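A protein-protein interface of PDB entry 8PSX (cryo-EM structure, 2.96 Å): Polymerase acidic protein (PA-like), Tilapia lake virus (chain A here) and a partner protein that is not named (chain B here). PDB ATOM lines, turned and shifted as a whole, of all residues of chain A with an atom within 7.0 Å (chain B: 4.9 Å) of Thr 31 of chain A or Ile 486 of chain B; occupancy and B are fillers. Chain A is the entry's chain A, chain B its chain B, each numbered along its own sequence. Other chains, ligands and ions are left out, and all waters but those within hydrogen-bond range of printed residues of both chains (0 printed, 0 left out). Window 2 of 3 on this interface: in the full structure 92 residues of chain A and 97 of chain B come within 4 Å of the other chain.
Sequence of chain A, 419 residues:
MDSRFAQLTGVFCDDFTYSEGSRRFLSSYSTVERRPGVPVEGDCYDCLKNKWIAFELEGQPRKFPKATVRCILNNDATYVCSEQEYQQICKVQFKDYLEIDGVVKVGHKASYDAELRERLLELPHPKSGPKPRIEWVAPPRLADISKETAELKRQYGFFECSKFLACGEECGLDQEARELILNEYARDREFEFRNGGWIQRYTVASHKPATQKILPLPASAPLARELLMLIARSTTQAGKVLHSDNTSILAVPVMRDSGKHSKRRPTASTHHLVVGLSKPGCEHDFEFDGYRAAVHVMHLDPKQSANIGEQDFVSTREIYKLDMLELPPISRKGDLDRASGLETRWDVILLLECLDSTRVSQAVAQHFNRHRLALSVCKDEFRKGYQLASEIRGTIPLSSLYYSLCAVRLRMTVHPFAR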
ATOM      1  N   SER A  27     -21.408  34.535 -12.487  1.00  0.00           N
ATOM      2  CA  SER A  27     -21.229  34.199 -11.082  1.00  0.00           C
ATOM      3  C   SER A  27     -19.762  34.326 -10.691  1.00  0.00           C
ATOM      4  O   SER A  27     -18.879  33.811 -11.382  1.00  0.00           O
ATOM      5  CB  SER A  27     -21.729  32.781 -10.814  1.00  0.00           C
ATOM      6  OG  SER A  27     -21.458  32.385  -9.483  1.00  0.00           O
ATOM      7  N   SER A  28     -19.505  35.013  -9.574  1.00  0.00           N
ATOM      8  CA  SER A  28     -18.138  35.189  -9.101  1.00  0.00           C
ATOM      9  C   SER A  28     -17.521  33.886  -8.611  1.00  0.00           C
ATOM     10  O   SER A  28     -16.300  33.818  -8.445  1.00  0.00           O
ATOM     11  CB  SER A  28     -18.096  36.226  -7.980  1.00  0.00           C
ATOM     12  OG  SER A  28     -18.213  37.541  -8.492  1.00  0.00           O
ATOM     13  N   TYR A  29     -18.334  32.861  -8.365  1.00  0.00           N
ATOM     14  CA  TYR A  29     -17.847  31.568  -7.905  1.00  0.00           C
ATOM     15  C   TYR A  29     -17.635  30.580  -9.040  1.00  0.00           C
ATOM     16  O   TYR A  29     -17.274  29.429  -8.780  1.00  0.00           O
ATOM     17  CB  TYR A  29     -18.823  30.974  -6.889  1.00  0.00           C
ATOM     18  CG  TYR A  29     -19.188  31.927  -5.780  1.00  0.00           C
ATOM     19  CD1 TYR A  29     -20.274  32.782  -5.902  1.00  0.00           C
ATOM     20  CD2 TYR A  29     -18.443  31.980  -4.612  1.00  0.00           C
ATOM     21  CE1 TYR A  29     -20.609  33.657  -4.893  1.00  0.00           C
ATOM     22  CE2 TYR A  29     -18.772  32.850  -3.598  1.00  0.00           C
ATOM     23  CZ  TYR A  29     -19.856  33.687  -3.744  1.00  0.00           C
ATOM     24  OH  TYR A  29     -20.189  34.560  -2.735  1.00  0.00           O
ATOM     25  N   SER A  30     -17.848  30.995 -10.284  1.00  0.00           N
ATOM     26  CA  SER A  30     -17.691  30.126 -11.440  1.00  0.00           C
ATOM     27  C   SER A  30     -16.355  30.414 -12.107  1.00  0.00           C
ATOM     28  O   SER A  30     -16.056  31.564 -12.444  1.00  0.00           O
ATOM     29  CB  SER A  30     -18.835  30.330 -12.433  1.00  0.00           C
ATOM     30  OG  SER A  30     -18.562  29.681 -13.660  1.00  0.00           O
ATOM     31  N   THR A  31     -15.555  29.366 -12.295  1.00  0.00           N
ATOM     32  CA  THR A  31     -14.243  29.507 -12.911  1.00  0.00           C
ATOM     33  C   THR A  31     -14.319  29.734 -14.414  1.00  0.00           C
ATOM     34  O   THR A  31     -13.297  30.069 -15.025  1.00  0.00           O
ATOM     35  CB  THR A  31     -13.399  28.264 -12.624  1.00  0.00           C
ATOM     36  OG1 THR A  31     -13.811  27.684 -11.380  1.00  0.00           O
ATOM     37  CG2 THR A  31     -11.928  28.625 -12.546  1.00  0.00           C
ATOM     38  N   VAL A  32     -15.488  29.560 -15.021  1.00  0.00           N
ATOM     39  CA  VAL A  32     -15.670  29.787 -16.447  1.00  0.00           C
ATOM     40  C   VAL A  32     -16.383  31.106 -16.718  1.00  0.00           C
ATOM     41  O   VAL A  32     -16.036  31.816 -17.662  1.00  0.00           O
ATOM     42  CB  VAL A  32     -16.437  28.602 -17.072  1.00  0.00           C
ATOM     43  CG1 VAL A  32     -16.794  28.893 -18.522  1.00  0.00           C
ATOM     44  CG2 VAL A  32     -15.614  27.330 -16.971  1.00  0.00           C
ATOM     45  N   GLU A  33     -17.379  31.447 -15.898  1.00  0.00           N
ATOM     46  CA  GLU A  33     -18.153  32.663 -16.109  1.00  0.00           C
ATOM     47  C   GLU A  33     -17.467  33.907 -15.560  1.00  0.00           C
ATOM     48  O   GLU A  33     -17.864  35.021 -15.915  1.00  0.00           O
ATOM     49  CB  GLU A  33     -19.534  32.516 -15.471  1.00  0.00           C
ATOM     50  CG  GLU A  33     -20.429  31.515 -16.176  1.00  0.00           C
ATOM     51  CD  GLU A  33     -21.446  30.888 -15.246  1.00  0.00           C
ATOM     52  OE1 GLU A  33     -22.031  31.619 -14.420  1.00  0.00           O
ATOM     53  OE2 GLU A  33     -21.660  29.660 -15.341  1.00  0.00           O
ATOM     54  N   ARG A  34     -16.455  33.747 -14.713  1.00  0.00           N
ATOM     55  CA  ARG A  34     -15.713  34.899 -14.216  1.00  0.00           C
ATOM     56  C   ARG A  34     -15.044  35.630 -15.370  1.00  0.00           C
ATOM     57  O   ARG A  34     -14.593  35.014 -16.339  1.00  0.00           O
ATOM     58  CB  ARG A  34     -14.653  34.453 -13.210  1.00  0.00           C
ATOM     59  CG  ARG A  34     -15.088  34.504 -11.760  1.00  0.00           C
ATOM     60  CD  ARG A  34     -14.024  33.896 -10.865  1.00  0.00           C
ATOM     61  NE  ARG A  34     -13.053  34.886 -10.411  1.00  0.00           N
ATOM     62  CZ  ARG A  34     -13.064  35.469  -9.219  1.00  0.00           C
ATOM     63  NH1 ARG A  34     -13.991  35.191  -8.318  1.00  0.00           N
ATOM     64  NH2 ARG A  34     -12.116  36.354  -8.924  1.00  0.00           N
ATOM     65  N   LEU B 468      -3.374  31.206 -14.433  1.00  0.00           N
ATOM     66  CA  LEU B 468      -4.674  31.670 -13.974  1.00  0.00           C
ATOM     67  C   LEU B 468      -4.631  33.159 -13.660  1.00  0.00           C
ATOM     68  O   LEU B 468      -3.566  33.761 -13.515  1.00  0.00           O
ATOM     69  CB  LEU B 468      -5.124  30.902 -12.728  1.00  0.00           C
ATOM     70  CG  LEU B 468      -5.502  29.433 -12.901  1.00  0.00           C
ATOM     71  CD1 LEU B 468      -5.829  28.831 -11.548  1.00  0.00           C
ATOM     72  CD2 LEU B 468      -6.682  29.300 -13.853  1.00  0.00           C
ATOM     73  N   VAL B 472      -7.988  34.897  -8.718  1.00  0.00           N
ATOM     74  CA  VAL B 472      -8.954  33.817  -8.541  1.00  0.00           C
ATOM     75  C   VAL B 472      -8.557  32.994  -7.319  1.00  0.00           C
ATOM     76  O   VAL B 472      -7.426  32.492  -7.261  1.00  0.00           O
ATOM     77  CB  VAL B 472      -9.040  32.933  -9.794  1.00  0.00           C
ATOM     78  CG1 VAL B 472      -9.801  31.658  -9.488  1.00  0.00           C
ATOM     79  CG2 VAL B 472      -9.706  33.688 -10.929  1.00  0.00           C
ATOM     80  N   LEU B 476     -12.042  27.476  -5.572  1.00  0.00           N
ATOM     81  CA  LEU B 476     -13.143  27.329  -6.510  1.00  0.00           C
ATOM     82  C   LEU B 476     -13.091  25.962  -7.188  1.00  0.00           C
ATOM     83  O   LEU B 476     -12.034  25.339  -7.316  1.00  0.00           O
ATOM     84  CB  LEU B 476     -13.106  28.436  -7.562  1.00  0.00           C
ATOM     85  CG  LEU B 476     -13.253  29.871  -7.050  1.00  0.00           C
ATOM     86  CD1 LEU B 476     -13.313  30.841  -8.216  1.00  0.00           C
ATOM     87  CD2 LEU B 476     -14.484  30.024  -6.170  1.00  0.00           C
ATOM     88  N   LEU B 477     -14.256  25.500  -7.632  1.00  0.00           N
ATOM     89  CA  LEU B 477     -14.385  24.183  -8.238  1.00  0.00           C
ATOM     90  C   LEU B 477     -14.199  24.262  -9.748  1.00  0.00           C
ATOM     91  O   LEU B 477     -14.639  25.219 -10.392  1.00  0.00           O
ATOM     92  CB  LEU B 477     -15.752  23.579  -7.915  1.00  0.00           C
ATOM     93  CG  LEU B 477     -16.116  23.517  -6.430  1.00  0.00           C
ATOM     94  CD1 LEU B 477     -17.497  22.915  -6.248  1.00  0.00           C
ATOM     95  CD2 LEU B 477     -15.076  22.730  -5.656  1.00  0.00           C
ATOM     96  N   VAL B 478     -13.544  23.248 -10.307  1.00  0.00           N
ATOM     97  CA  VAL B 478     -13.304  23.158 -11.743  1.00  0.00           C
ATOM     98  C   VAL B 478     -13.576  21.732 -12.196  1.00  0.00           C
ATOM     99  O   VAL B 478     -13.153  20.771 -11.546  1.00  0.00           O
ATOM    100  CB  VAL B 478     -11.865  23.573 -12.114  1.00  0.00           C
ATOM    101  CG1 VAL B 478     -11.583  24.992 -11.659  1.00  0.00           C
ATOM    102  CG2 VAL B 478     -10.855  22.604 -11.517  1.00  0.00           C
ATOM    103  N   ASP B 482     -14.600  22.735 -17.639  1.00  0.00           N
ATOM    104  CA  ASP B 482     -14.179  24.046 -17.162  1.00  0.00           C
ATOM    105  C   ASP B 482     -12.695  24.275 -17.418  1.00  0.00           C
ATOM    106  O   ASP B 482     -12.293  25.365 -17.839  1.00  0.00           O
ATOM    107  CB  ASP B 482     -14.482  24.188 -15.672  1.00  0.00           C
ATOM    108  CG  ASP B 482     -15.967  24.239 -15.380  1.00  0.00           C
ATOM    109  OD1 ASP B 482     -16.713  23.408 -15.940  1.00  0.00           O
ATOM    110  OD2 ASP B 482     -16.387  25.109 -14.588  1.00  0.00           O
ATOM    111  N   VAL B 483     -11.866  23.264 -17.156  1.00  0.00           N
ATOM    112  CA  VAL B 483     -10.432  23.405 -17.398  1.00  0.00           C
ATOM    113  C   VAL B 483     -10.170  23.663 -18.874  1.00  0.00           C
ATOM    114  O   VAL B 483      -9.391  24.555 -19.238  1.00  0.00           O
ATOM    115  CB  VAL B 483      -9.682  22.155 -16.898  1.00  0.00           C
ATOM    116  CG1 VAL B 483      -8.225  22.188 -17.339  1.00  0.00           C
ATOM    117  CG2 VAL B 483      -9.783  22.045 -15.385  1.00  0.00           C
ATOM    118  N   SER B 484     -10.820  22.891 -19.749  1.00  0.00           N
ATOM    119  CA  SER B 484     -10.620  23.091 -21.180  1.00  0.00           C
ATOM    120  C   SER B 484     -11.057  24.487 -21.606  1.00  0.00           C
ATOM    121  O   SER B 484     -10.365  25.151 -22.385  1.00  0.00           O
ATOM    122  CB  SER B 484     -11.379  22.027 -21.971  1.00  0.00           C
ATOM    123  OG  SER B 484     -12.580  21.669 -21.315  1.00  0.00           O
ATOM    124  N   LYS B 485     -12.203  24.952 -21.102  1.00  0.00           N
ATOM    125  CA  LYS B 485     -12.704  26.268 -21.484  1.00  0.00           C
ATOM    126  C   LYS B 485     -11.783  27.380 -20.995  1.00  0.00           C
ATOM    127  O   LYS B 485     -11.529  28.346 -21.723  1.00  0.00           O
ATOM    128  CB  LYS B 485     -14.118  26.462 -20.939  1.00  0.00           C
ATOM    129  CG  LYS B 485     -15.195  25.791 -21.778  1.00  0.00           C
ATOM    130  CD  LYS B 485     -16.573  26.357 -21.485  1.00  0.00           C
ATOM    131  CE  LYS B 485     -17.572  25.262 -21.141  1.00  0.00           C
ATOM    132  NZ  LYS B 485     -17.360  24.713 -19.773  1.00  0.00           N
ATOM    133  N   ILE B 486     -11.277  27.266 -19.767  1.00  0.00           N
ATOM    134  CA  ILE B 486     -10.371  28.281 -19.240  1.00  0.00           C
ATOM    135  C   ILE B 486      -9.086  28.316 -20.055  1.00  0.00           C
ATOM    136  O   ILE B 486      -8.583  29.393 -20.409  1.00  0.00           O
ATOM    137  CB  ILE B 486     -10.090  28.017 -17.749  1.00  0.00           C
ATOM    138  CG1 ILE B 486     -11.381  28.119 -16.932  1.00  0.00           C
ATOM    139  CG2 ILE B 486      -9.059  28.999 -17.216  1.00  0.00           C
ATOM    140  CD1 ILE B 486     -11.368  27.281 -15.673  1.00  0.00           C
ATOM    141  N   ARG B 487      -8.534  27.142 -20.370  1.00  0.00           N
ATOM    142  CA  ARG B 487      -7.328  27.090 -21.188  1.00  0.00           C
ATOM    143  C   ARG B 487      -7.571  27.708 -22.559  1.00  0.00           C
ATOM    144  O   ARG B 487      -6.735  28.468 -23.063  1.00  0.00           O
ATOM    145  CB  ARG B 487      -6.861  25.641 -21.329  1.00  0.00           C
ATOM    146  CG  ARG B 487      -5.474  25.473 -21.923  1.00  0.00           C
ATOM    147  CD  ARG B 487      -4.395  26.044 -21.017  1.00  0.00           C
ATOM    148  NE  ARG B 487      -3.120  25.353 -21.183  1.00  0.00           N
ATOM    149  CZ  ARG B 487      -2.419  25.318 -22.308  1.00  0.00           C
ATOM    150  NH1 ARG B 487      -2.823  25.951 -23.398  1.00  0.00           N
ATOM    151  NH2 ARG B 487      -1.280  24.632 -22.341  1.00  0.00           N
ATOM    152  N   ALA B 488      -8.711  27.394 -23.179  1.00  0.00           N
ATOM    153  CA  ALA B 488      -9.015  27.941 -24.497  1.00  0.00           C
ATOM    154  C   ALA B 488      -9.157  29.456 -24.449  1.00  0.00           C
ATOM    155  O   ALA B 488      -8.661  30.161 -25.336  1.00  0.00           O
ATOM    156  CB  ALA B 488     -10.290  27.302 -25.043  1.00  0.00           C
ATOM    157  N   ALA B 489      -9.840  29.976 -23.427  1.00  0.00           N
ATOM    158  CA  ALA B 489     -10.001  31.422 -23.311  1.00  0.00           C
ATOM    159  C   ALA B 489      -8.656  32.110 -23.128  1.00  0.00           C
ATOM    160  O   ALA B 489      -8.387  33.145 -23.751  1.00  0.00           O
ATOM    161  CB  ALA B 489     -10.935  31.755 -22.151  1.00  0.00           C
ATOM    162  N   ARG B 490      -7.793  31.548 -22.278  1.00  0.00           N
ATOM    163  CA  ARG B 490      -6.480  32.152 -22.081  1.00  0.00           C
ATOM    164  C   ARG B 490      -5.653  32.096 -23.359  1.00  0.00           C
ATOM    165  O   ARG B 490      -4.936  33.050 -23.683  1.00  0.00           O
ATOM    166  CB  ARG B 490      -5.748  31.459 -20.932  1.00  0.00           C
ATOM    167  CG  ARG B 490      -4.382  32.054 -20.615  1.00  0.00           C
ATOM    168  CD  ARG B 490      -4.466  33.541 -20.304  1.00  0.00           C
ATOM    169  NE  ARG B 490      -3.183  34.080 -19.871  1.00  0.00           N
ATOM    170  CZ  ARG B 490      -2.976  35.345 -19.533  1.00  0.00           C
ATOM    171  NH1 ARG B 490      -3.950  36.239 -19.564  1.00  0.00           N
ATOM    172  NH2 ARG B 490      -1.758  35.723 -19.156  1.00  0.00           N
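Thr 31 of chain A touches just these residues of chain B: Leu 476, Leu 477, Val 478 and Ile 486. Ile 486 of chain B touches one residue of chain A. Printed residues of chain A within 4 Å of Leu 477 of chain B: Thr 31. Of the printed residues of chain B, Arg 34 of chain A touches Val 472 (3.6 Å). Printed residues of chain A within 4 Å of Leu 476 of chain B: Tyr 29 and Thr 31. Of the printed residues of chain A, Val 478 of chain B touches Thr 31. Ala 488 of chain B touches none of the printed residues of chain A.
Of the 14 printed residues of chain B, 7 touch a printed residue of chain A. Among the printed residues, no Asp or Glu carboxylate lies within 4 Å of a Lys or Arg side-chain nitrogen of the other chain.
Among the printed residues, pairs that only touch across the chains: Thr 31 of chain A with Ile 486 of chain B (3.3 Å), Val 32 of chain A with Asp 482 of chain B (3.3 Å), Thr 31 of chain A with Val 478 of chain B (3.5 Å), Arg 34 of chain A with Val 472 of chain B (3.6 Å), Tyr 29 of chain A with Leu 476 of chain B (3.9 Å), Val 32 of chain A with Lys 485 of chain B (3.9 Å) and Thr 31 of chain A with Leu 476 of chain B (3.95 Å).
O of Leu 477 of chain B is in hydrogen-bond range of OG1 of Thr 31 of chain A, at 2.8 Å.
The side-chain hydroxyl of Ser 27 of chain A sits close to the backbone NH of Tyr 29 of chain A (3.4 Å). The backbone carbonyl oxygen of Ser 28 of chain A is in hydrogen-bond range of the guanidinium group of Arg 34 of chain A, 2.7 Å away. N of Val 32 of chain A lies close to OG of Ser 30 of chain A, 3.4 Å away.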
